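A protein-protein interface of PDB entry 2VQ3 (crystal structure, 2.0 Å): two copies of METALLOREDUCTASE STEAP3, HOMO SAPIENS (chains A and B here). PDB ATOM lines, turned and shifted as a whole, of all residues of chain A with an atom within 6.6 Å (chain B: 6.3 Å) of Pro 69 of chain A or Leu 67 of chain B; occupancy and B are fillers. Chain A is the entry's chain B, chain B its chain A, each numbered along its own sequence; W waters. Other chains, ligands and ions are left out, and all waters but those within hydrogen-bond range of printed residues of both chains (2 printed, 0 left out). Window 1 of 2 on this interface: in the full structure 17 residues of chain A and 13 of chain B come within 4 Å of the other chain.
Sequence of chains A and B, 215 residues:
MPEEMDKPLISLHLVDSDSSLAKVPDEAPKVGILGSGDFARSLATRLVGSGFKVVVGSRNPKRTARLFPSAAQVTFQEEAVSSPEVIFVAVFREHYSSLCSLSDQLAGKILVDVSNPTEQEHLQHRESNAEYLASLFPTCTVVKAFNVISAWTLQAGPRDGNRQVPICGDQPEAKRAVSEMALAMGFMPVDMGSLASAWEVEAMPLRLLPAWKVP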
ATOM      1  N   ALA A  40      -5.175 -20.598  16.159  1.00  0.00           N
ATOM      2  CA  ALA A  40      -4.708 -19.721  15.100  1.00  0.00           C
ATOM      3  C   ALA A  40      -3.202 -19.882  14.996  1.00  0.00           C
ATOM      4  O   ALA A  40      -2.673 -20.036  13.923  1.00  0.00           O
ATOM      5  CB  ALA A  40      -5.103 -18.325  15.333  1.00  0.00           C
ATOM      6  N   ARG A  41      -2.514 -19.787  16.120  1.00  0.00           N
ATOM      7  CA  ARG A  41      -1.088 -19.569  16.117  1.00  0.00           C
ATOM      8  C   ARG A  41      -0.426 -20.914  15.705  1.00  0.00           C
ATOM      9  O   ARG A  41       0.571 -20.938  15.017  1.00  0.00           O
ATOM     10  CB  ARG A  41      -0.604 -19.106  17.488  1.00  0.00           C
ATOM     11  CG  ARG A  41       0.869 -18.829  17.574  1.00  0.00           C
ATOM     12  CD  ARG A  41       1.301 -18.329  18.957  1.00  0.00           C
ATOM     13  NE  ARG A  41       1.503 -19.425  19.895  1.00  0.00           N
ATOM     14  CZ  ARG A  41       0.656 -19.705  20.863  1.00  0.00           C
ATOM     15  NH1 ARG A  41      -0.408 -18.950  21.023  1.00  0.00           N
ATOM     16  NH2 ARG A  41       0.870 -20.709  21.686  1.00  0.00           N
ATOM     17  N   SER A  42      -1.014 -22.020  16.142  1.00  0.00           N
ATOM     18  CA  SER A  42      -0.511 -23.335  15.798  1.00  0.00           C
ATOM     19  C   SER A  42      -0.725 -23.667  14.314  1.00  0.00           C
ATOM     20  O   SER A  42       0.176 -24.170  13.680  1.00  0.00           O
ATOM     21  CB  SER A  42      -1.065 -24.395  16.752  1.00  0.00           C
ATOM     22  OG  SER A  42      -0.796 -24.061  18.100  1.00  0.00           O
ATOM     23  N   ALA A  44      -0.961 -21.398  11.947  1.00  0.00           N
ATOM     24  CA  ALA A  44      -0.012 -20.529  11.253  1.00  0.00           C
ATOM     25  C   ALA A  44       1.373 -21.187  11.200  1.00  0.00           C
ATOM     26  O   ALA A  44       2.040 -21.190  10.146  1.00  0.00           O
ATOM     27  CB  ALA A  44       0.079 -19.162  11.925  1.00  0.00           C
ATOM     28  N   THR A  45       1.784 -21.762  12.336  1.00  0.00           N
ATOM     29  CA  THR A  45       3.088 -22.404  12.452  1.00  0.00           C
ATOM     30  C   THR A  45       3.183 -23.579  11.473  1.00  0.00           C
ATOM     31  O   THR A  45       4.151 -23.711  10.743  1.00  0.00           O
ATOM     32  CB  THR A  45       3.383 -22.862  13.898  1.00  0.00           C
ATOM     33  OG1 THR A  45       3.276 -21.742  14.802  1.00  0.00           O
ATOM     34  CG2 THR A  45       4.787 -23.445  13.999  1.00  0.00           C
ATOM     35  N   ARG A  46       2.147 -24.401  11.433  1.00  0.00           N
ATOM     36  CA  ARG A  46       2.147 -25.578  10.565  1.00  0.00           C
ATOM     37  C   ARG A  46       2.120 -25.192   9.086  1.00  0.00           C
ATOM     38  O   ARG A  46       2.848 -25.736   8.279  1.00  0.00           O
ATOM     39  CB  ARG A  46       0.981 -26.509  10.893  1.00  0.00           C
ATOM     40  CG  ARG A  46       1.045 -27.868  10.213  1.00  0.00           C
ATOM     41  CD  ARG A  46       2.256 -28.659  10.697  1.00  0.00           C
ATOM     42  NE  ARG A  46       2.151 -30.078  10.400  1.00  0.00           N
ATOM     43  CZ  ARG A  46       2.531 -31.054  11.218  1.00  0.00           C
ATOM     44  NH1 ARG A  46       3.042 -30.770  12.412  1.00  0.00           N
ATOM     45  NH2 ARG A  46       2.396 -32.324  10.849  1.00  0.00           N
ATOM     46  N   VAL A  48       3.117 -22.323   7.626  1.00  0.00           N
ATOM     47  CA  VAL A  48       4.430 -21.745   7.292  1.00  0.00           C
ATOM     48  C   VAL A  48       5.485 -22.848   7.128  1.00  0.00           C
ATOM     49  O   VAL A  48       6.296 -22.807   6.206  1.00  0.00           O
ATOM     50  CB  VAL A  48       4.895 -20.720   8.380  1.00  0.00           C
ATOM     51  CG1 VAL A  48       6.357 -20.360   8.194  1.00  0.00           C
ATOM     52  CG2 VAL A  48       4.027 -19.480   8.327  1.00  0.00           C
ATOM     53  N   GLY A  49       5.470 -23.837   8.021  1.00  0.00           N
ATOM     54  CA  GLY A  49       6.423 -24.953   7.920  1.00  0.00           C
ATOM     55  C   GLY A  49       6.192 -25.876   6.727  1.00  0.00           C
ATOM     56  O   GLY A  49       7.053 -26.681   6.369  1.00  0.00           O
ATOM     57  N   SER A  50       5.023 -25.746   6.117  1.00  0.00           N
ATOM     58  CA  SER A  50       4.610 -26.542   4.976  1.00  0.00           C
ATOM     59  C   SER A  50       4.676 -25.762   3.666  1.00  0.00           C
ATOM     60  O   SER A  50       4.176 -26.229   2.659  1.00  0.00           O
ATOM     61  CB  SER A  50       3.174 -27.017   5.208  1.00  0.00           C
ATOM     62  OG  SER A  50       3.079 -27.688   6.455  1.00  0.00           O
ATOM     63  N   ALA A  65       0.899 -10.072  16.818  1.00  0.00           N
ATOM     64  CA  ALA A  65       2.036 -10.395  15.958  1.00  0.00           C
ATOM     65  C   ALA A  65       3.257 -10.881  16.751  1.00  0.00           C
ATOM     66  O   ALA A  65       3.997 -11.741  16.295  1.00  0.00           O
ATOM     67  CB  ALA A  65       2.415  -9.193  15.082  1.00  0.00           C
ATOM     68  N   ARG A  66       3.458 -10.325  17.940  1.00  0.00           N
ATOM     69  CA  ARG A  66       4.643 -10.630  18.758  1.00  0.00           C
ATOM     70  C   ARG A  66       4.851 -12.134  19.018  1.00  0.00           C
ATOM     71  O   ARG A  66       5.987 -12.601  19.029  1.00  0.00           O
ATOM     72  CB  ARG A  66       4.584  -9.846  20.065  1.00  0.00           C
ATOM     73  CG  ARG A  66       4.675  -8.337  19.845  1.00  0.00           C
ATOM     74  CD  ARG A  66       4.627  -7.526  21.129  1.00  0.00           C
ATOM     75  NE  ARG A  66       5.847  -7.653  21.927  1.00  0.00           N
ATOM     76  CZ  ARG A  66       5.984  -8.451  22.984  1.00  0.00           C
ATOM     77  NH1 ARG A  66       4.983  -9.239  23.391  1.00  0.00           N
ATOM     78  NH2 ARG A  66       7.143  -8.487  23.634  1.00  0.00           N
ATOM     79  N   LEU A  67       3.761 -12.873  19.203  1.00  0.00           N
ATOM     80  CA  LEU A  67       3.814 -14.317  19.496  1.00  0.00           C
ATOM     81  C   LEU A  67       3.773 -15.211  18.260  1.00  0.00           C
ATOM     82  O   LEU A  67       4.159 -16.372  18.332  1.00  0.00           O
ATOM     83  CB  LEU A  67       2.663 -14.730  20.418  1.00  0.00           C
ATOM     84  CG  LEU A  67       2.741 -14.215  21.855  1.00  0.00           C
ATOM     85  CD1 LEU A  67       2.546 -12.720  21.864  1.00  0.00           C
ATOM     86  CD2 LEU A  67       1.696 -14.914  22.758  1.00  0.00           C
ATOM     87  N   PHE A  68       3.295 -14.682  17.135  1.00  0.00           N
ATOM     88  CA  PHE A  68       3.127 -15.493  15.924  1.00  0.00           C
ATOM     89  C   PHE A  68       4.447 -15.759  15.193  1.00  0.00           C
ATOM     90  O   PHE A  68       5.369 -14.955  15.281  1.00  0.00           O
ATOM     91  CB  PHE A  68       2.134 -14.814  14.972  1.00  0.00           C
ATOM     92  CG  PHE A  68       0.720 -15.255  15.186  1.00  0.00           C
ATOM     93  CD1 PHE A  68       0.090 -15.027  16.394  1.00  0.00           C
ATOM     94  CD2 PHE A  68       0.034 -15.942  14.196  1.00  0.00           C
ATOM     95  CE1 PHE A  68      -1.234 -15.452  16.599  1.00  0.00           C
ATOM     96  CE2 PHE A  68      -1.269 -16.372  14.405  1.00  0.00           C
ATOM     97  CZ  PHE A  68      -1.895 -16.136  15.601  1.00  0.00           C
ATOM     98  N   PRO A  69       4.530 -16.872  14.440  1.00  0.00           N
ATOM     99  CA  PRO A  69       5.721 -17.144  13.637  1.00  0.00           C
ATOM    100  C   PRO A  69       6.025 -15.962  12.723  1.00  0.00           C
ATOM    101  O   PRO A  69       5.101 -15.409  12.132  1.00  0.00           O
ATOM    102  CB  PRO A  69       5.335 -18.384  12.825  1.00  0.00           C
ATOM    103  CG  PRO A  69       3.869 -18.511  12.970  1.00  0.00           C
ATOM    104  CD  PRO A  69       3.527 -17.931  14.288  1.00  0.00           C
ATOM    105  N   SER A  70       7.293 -15.560  12.636  1.00  0.00           N
ATOM    106  CA  SER A  70       7.671 -14.339  11.895  1.00  0.00           C
ATOM    107  C   SER A  70       7.257 -14.373  10.441  1.00  0.00           C
ATOM    108  O   SER A  70       6.948 -13.333   9.853  1.00  0.00           O
ATOM    109  CB  SER A  70       9.169 -14.078  11.935  1.00  0.00           C
ATOM    110  OG  SER A  70       9.667 -14.370  13.211  1.00  0.00           O
ATOM    111  N   ALA A  71       7.274 -15.562   9.855  1.00  0.00           N
ATOM    112  CA  ALA A  71       6.931 -15.724   8.448  1.00  0.00           C
ATOM    113  C   ALA A  71       5.458 -15.431   8.162  1.00  0.00           C
ATOM    114  O   ALA A  71       5.100 -15.179   7.015  1.00  0.00           O
ATOM    115  CB  ALA A  71       7.306 -17.106   7.969  1.00  0.00           C
ATOM    116  N   ALA A  72       4.595 -15.474   9.180  1.00  0.00           N
ATOM    117  CA  ALA A  72       3.200 -15.083   9.012  1.00  0.00           C
ATOM    118  C   ALA A  72       3.068 -13.553   9.085  1.00  0.00           C
ATOM    119  O   ALA A  72       3.754 -12.896   9.876  1.00  0.00           O
ATOM    120  CB  ALA A  72       2.317 -15.742  10.076  1.00  0.00           C
ATOM    121  N   GLN A  73       2.210 -12.993   8.243  1.00  0.00           N
ATOM    122  CA  GLN A  73       1.913 -11.575   8.279  1.00  0.00           C
ATOM    123  C   GLN A  73       0.628 -11.338   9.076  1.00  0.00           C
ATOM    124  O   GLN A  73      -0.468 -11.668   8.626  1.00  0.00           O
ATOM    125  CB  GLN A  73       1.782 -11.020   6.855  1.00  0.00           C
ATOM    126  CG  GLN A  73       3.113 -10.950   6.106  1.00  0.00           C
ATOM    127  CD  GLN A  73       2.968 -10.321   4.734  1.00  0.00           C
ATOM    128  OE1 GLN A  73       1.852 -10.172   4.222  1.00  0.00           O
ATOM    129  NE2 GLN A  73       4.084  -9.940   4.129  1.00  0.00           N
ATOM    130  N   VAL A  74       0.773 -10.784  10.272  1.00  0.00           N
ATOM    131  CA  VAL A  74      -0.362 -10.535  11.140  1.00  0.00           C
ATOM    132  C   VAL A  74      -0.820  -9.107  10.906  1.00  0.00           C
ATOM    133  O   VAL A  74      -0.028  -8.177  11.002  1.00  0.00           O
ATOM    134  CB  VAL A  74      -0.020 -10.709  12.648  1.00  0.00           C
ATOM    135  CG1 VAL A  74      -1.257 -10.433  13.489  1.00  0.00           C
ATOM    136  CG2 VAL A  74       0.538 -12.102  12.938  1.00  0.00           C
ATOM    137  N   ARG B  41      11.455 -22.981  20.858  1.00  0.00           N
ATOM    138  CA  ARG B  41      10.493 -22.131  20.191  1.00  0.00           C
ATOM    139  C   ARG B  41       9.399 -21.828  21.242  1.00  0.00           C
ATOM    140  O   ARG B  41       8.915 -20.718  21.352  1.00  0.00           O
ATOM    141  CB  ARG B  41       9.935 -22.876  18.979  1.00  0.00           C
ATOM    142  CG  ARG B  41       8.941 -22.141  18.136  1.00  0.00           C
ATOM    143  CD  ARG B  41       8.824 -22.798  16.783  1.00  0.00           C
ATOM    144  NE  ARG B  41       8.318 -24.160  16.889  1.00  0.00           N
ATOM    145  CZ  ARG B  41       7.081 -24.421  17.235  1.00  0.00           C
ATOM    146  NH1 ARG B  41       6.281 -23.410  17.436  1.00  0.00           N
ATOM    147  NH2 ARG B  41       6.645 -25.658  17.347  1.00  0.00           N
ATOM    148  N   ARG B  63      16.450 -19.757   8.217  1.00  0.00           N
ATOM    149  CA  ARG B  63      15.417 -20.753   8.186  1.00  0.00           C
ATOM    150  C   ARG B  63      14.633 -20.804   9.486  1.00  0.00           C
ATOM    151  O   ARG B  63      13.427 -20.886   9.497  1.00  0.00           O
ATOM    152  CB  ARG B  63      16.069 -22.077   7.928  1.00  0.00           C
ATOM    153  CG  ARG B  63      15.161 -23.251   7.992  1.00  0.00           C
ATOM    154  CD  ARG B  63      15.929 -24.463   7.573  1.00  0.00           C
ATOM    155  NE  ARG B  63      16.780 -24.151   6.425  1.00  0.00           N
ATOM    156  CZ  ARG B  63      16.745 -24.778   5.256  1.00  0.00           C
ATOM    157  NH1 ARG B  63      17.564 -24.399   4.283  1.00  0.00           N
ATOM    158  NH2 ARG B  63      15.905 -25.785   5.060  1.00  0.00           N
ATOM    159  N   THR B  64      15.356 -20.748  10.583  1.00  0.00           N
ATOM    160  CA  THR B  64      14.802 -20.909  11.919  1.00  0.00           C
ATOM    161  C   THR B  64      13.877 -19.767  12.333  1.00  0.00           C
ATOM    162  O   THR B  64      12.833 -19.988  12.924  1.00  0.00           O
ATOM    163  CB  THR B  64      15.954 -21.029  12.908  1.00  0.00           C
ATOM    164  OG1 THR B  64      16.562 -22.301  12.731  1.00  0.00           O
ATOM    165  CG2 THR B  64      15.463 -20.904  14.320  1.00  0.00           C
ATOM    166  N   ALA B  65      14.274 -18.554  12.008  1.00  0.00           N
ATOM    167  CA  ALA B  65      13.502 -17.372  12.333  1.00  0.00           C
ATOM    168  C   ALA B  65      12.047 -17.438  11.836  1.00  0.00           C
ATOM    169  O   ALA B  65      11.155 -16.974  12.495  1.00  0.00           O
ATOM    170  CB  ALA B  65      14.185 -16.141  11.804  1.00  0.00           C
ATOM    171  N   ARG B  66      11.831 -18.036  10.679  1.00  0.00           N
ATOM    172  CA  ARG B  66      10.504 -18.098  10.051  1.00  0.00           C
ATOM    173  C   ARG B  66       9.410 -18.634  10.992  1.00  0.00           C
ATOM    174  O   ARG B  66       8.279 -18.187  10.963  1.00  0.00           O
ATOM    175  CB  ARG B  66      10.561 -18.956   8.778  1.00  0.00           C
ATOM    176  CG  ARG B  66      11.428 -18.344   7.680  1.00  0.00           C
ATOM    177  CD  ARG B  66      11.506 -19.140   6.370  1.00  0.00           C
ATOM    178  NE  ARG B  66      10.427 -20.094   6.169  1.00  0.00           N
ATOM    179  CZ  ARG B  66       9.263 -19.824   5.602  1.00  0.00           C
ATOM    180  NH1 ARG B  66       8.984 -18.611   5.157  1.00  0.00           N
ATOM    181  NH2 ARG B  66       8.367 -20.783   5.487  1.00  0.00           N
ATOM    182  N   LEU B  67       9.772 -19.597  11.821  1.00  0.00           N
ATOM    183  CA  LEU B  67       8.807 -20.251  12.717  1.00  0.00           C
ATOM    184  C   LEU B  67       8.727 -19.653  14.127  1.00  0.00           C
ATOM    185  O   LEU B  67       7.784 -19.941  14.858  1.00  0.00           O
ATOM    186  CB  LEU B  67       9.121 -21.740  12.838  1.00  0.00           C
ATOM    187  CG  LEU B  67       9.005 -22.605  11.586  1.00  0.00           C
ATOM    188  CD1 LEU B  67       9.335 -24.058  11.957  1.00  0.00           C
ATOM    189  CD2 LEU B  67       7.637 -22.514  10.979  1.00  0.00           C
ATOM    190  N   PHE B  68       9.725 -18.857  14.503  1.00  0.00           N
ATOM    191  CA  PHE B  68       9.808 -18.313  15.867  1.00  0.00           C
ATOM    192  C   PHE B  68       8.896 -17.092  16.018  1.00  0.00           C
ATOM    193  O   PHE B  68       8.618 -16.417  15.038  1.00  0.00           O
ATOM    194  CB  PHE B  68      11.261 -17.977  16.255  1.00  0.00           C
ATOM    195  CG  PHE B  68      11.986 -19.109  16.942  1.00  0.00           C
ATOM    196  CD1 PHE B  68      12.269 -20.287  16.265  1.00  0.00           C
ATOM    197  CD2 PHE B  68      12.372 -19.003  18.279  1.00  0.00           C
ATOM    198  CE1 PHE B  68      12.935 -21.338  16.894  1.00  0.00           C
ATOM    199  CE2 PHE B  68      13.064 -20.058  18.922  1.00  0.00           C
ATOM    200  CZ  PHE B  68      13.321 -21.222  18.236  1.00  0.00           C
ATOM    201  N   PRO B  69       8.405 -16.834  17.251  1.00  0.00           N
ATOM    202  CA  PRO B  69       7.623 -15.626  17.521  1.00  0.00           C
ATOM    203  C   PRO B  69       8.372 -14.389  17.044  1.00  0.00           C
ATOM    204  O   PRO B  69       9.596 -14.320  17.217  1.00  0.00           O
ATOM    205  CB  PRO B  69       7.441 -15.640  19.052  1.00  0.00           C
ATOM    206  CG  PRO B  69       8.400 -16.666  19.565  1.00  0.00           C
ATOM    207  CD  PRO B  69       8.603 -17.645  18.463  1.00  0.00           C
ATOM    208  N   SER B  70       7.663 -13.452  16.403  1.00  0.00           N
ATOM    209  CA  SER B  70       8.306 -12.282  15.777  1.00  0.00           C
ATOM    210  C   SER B  70       9.093 -11.434  16.743  1.00  0.00           C
ATOM    211  O   SER B  70      10.089 -10.825  16.363  1.00  0.00           O
ATOM    212  CB  SER B  70       7.279 -11.369  15.122  1.00  0.00           C
ATOM    213  OG  SER B  70       6.319 -12.143  14.463  1.00  0.00           O
HETATM  214  O   HOH W   1      11.718 -14.447  15.304  1.00  0.00           O
HETATM  215  O   HOH W   2       4.107 -12.641  12.856  1.00  0.00           O
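Pro 69 of chain A touches just these residues of chain B: Arg 66, Leu 67 and Phe 68. Leu 67 of chain B touches just these residues of chain A: Thr 45, Val 48, Gly 49 and Pro 69. Printed residues of chain A within 4 Å of Ser 70 of chain B: Ala 65, Arg 66, Phe 68 and Ser 70. Printed residues of chain B within 4 Å of Phe 68 of chain A: Phe 68, Pro 69 and Ser 70. Of the printed residues of chain B, Val 48 of chain A touches Arg 66 (3.0 Å) and Leu 67 (3.7 Å). Of the printed residues of chain A, Phe 68 of chain B touches Phe 68, Pro 69 and Ser 70. Thr 64 of chain B touches none of the printed residues of chain A. Gln 73 of chain A touches none of the printed residues of chain B. The nearest residue of chain A that does not touch Leu 67 of chain B is Ser 70 of chain A (4.6 Å). The nearest printed residue of chain B that does not touch Leu 67 of chain A is Ser 70 of chain B (4.7 Å).
The backbone carbonyl oxygen of Ala 65 of chain A sits at hydrogen-bond distance from the side-chain hydroxyl of Ser 70 of chain B, at 3.0 Å. O of Ala 65 of chain B lies within hydrogen-bond range of OG of Ser 70 of chain A (3.1 Å). O of Arg 66 of chain A lies within hydrogen-bond range of N of Ser 70 of chain B, at 3.2 Å. O of Phe 68 of chain A is in hydrogen-bond range of N of Ser 70 of chain B (3.0 Å). The backbone NH (N) of Ser 70 of chain A lies within hydrogen-bond range of the backbone carbonyl oxygen (O) of Arg 66 of chain B (3.3 Å). The guanidinium group (NH2) of Arg 66 of chain B sits at hydrogen-bond distance from the backbone carbonyl oxygen (O) of Val 48 of chain A (3.0 Å). The backbone NH of Ala 71 of chain A lies within hydrogen-bond range of the backbone carbonyl oxygen of Arg 66 of chain B, at 3.0 Å. The backbone NH (N) of Ser 70 of chain A lies within hydrogen-bond range of the backbone carbonyl oxygen (O) of Phe 68 of chain B (2.9 Å).
Ala 65 of chain A touches Ser 70 of chain B, and with the chains exchanged Ser 70 of chain A touches Ala 65 of chain B. Leu 67 of chain A touches Pro 69 of chain B, and with the chains exchanged Pro 69 of chain A touches Leu 67 of chain B. Phe 68 of chain B touches its own counterpart, Phe 68 of chain A. Phe 68 of chain A touches Ser 70 of chain B, and with the chains exchanged Ser 70 of chain A touches Phe 68 of chain B. Of the 20 pairs that touch across the chains among the printed residues, 14 have their exchanged pair printed and touching as well.
Water W2 lies within hydrogen-bond range of the side-chain hydroxyl of Ser 70 of chain B, the backbone carbonyl oxygen of Ala 72 of chain A and the backbone carbonyl oxygen of Pro 69 of chain A. Water W1 bridges the backbone carbonyl oxygen of Pro 69 of chain B and the side-chain hydroxyl of Ser 70 of chain A.
Printed residues of chain A that touch a printed residue of chain B: Thr 45, Val 48, Gly 49, Ala 65, Arg 66, Leu 67, Phe 68, Pro 69, Ser 70 and Ala 71. Hydrophobic or aromatic side chains of chain A within 4 Å of the printed part of chain B: Val 48, Pro 69 and Ala 71. Of the 9 printed residues of chain B, 7 touch a printed residue of chain A. Printed residues of chain B that touch a printed residue of chain A: Arg 41, Ala 65, Arg 66, Leu 67, Phe 68, Pro 69 and Ser 70. Hydrophobic or aromatic side chains of chain B within 4 Å of the printed part of chain A: Leu 67 and Pro 69. Along chain B the printed residues that touch a printed residue of chain A span positions 41 to 70. Among the printed residues, 20 pairs touch across the chains.
O of Arg 41 of chain A is in hydrogen-bond range of OG1 of Thr 45 of chain A (2.8 Å).
Among the printed residues, merely in contact across the chains: Thr 45 of chain A with Arg 41 of chain B, Thr 45 of chain A with Leu 67 of chain B, Val 48 of chain A with Leu 67 of chain B, Gly 49 of chain A with Leu 67 of chain B, Arg 66 of chain A with Pro 69 of chain B, Leu 67 of chain A with Pro 69 of chain B, Phe 68 of chain A with Phe 68 of chain B, Phe 68 of chain A with Pro 69 of chain B, Pro 69 of chain A with Arg 66 of chain B, Pro 69 of chain A with Leu 67 of chain B, Pro 69 of chain A with Phe 68 of chain B and Ser 70 of chain A with Ser 70 of chain B.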
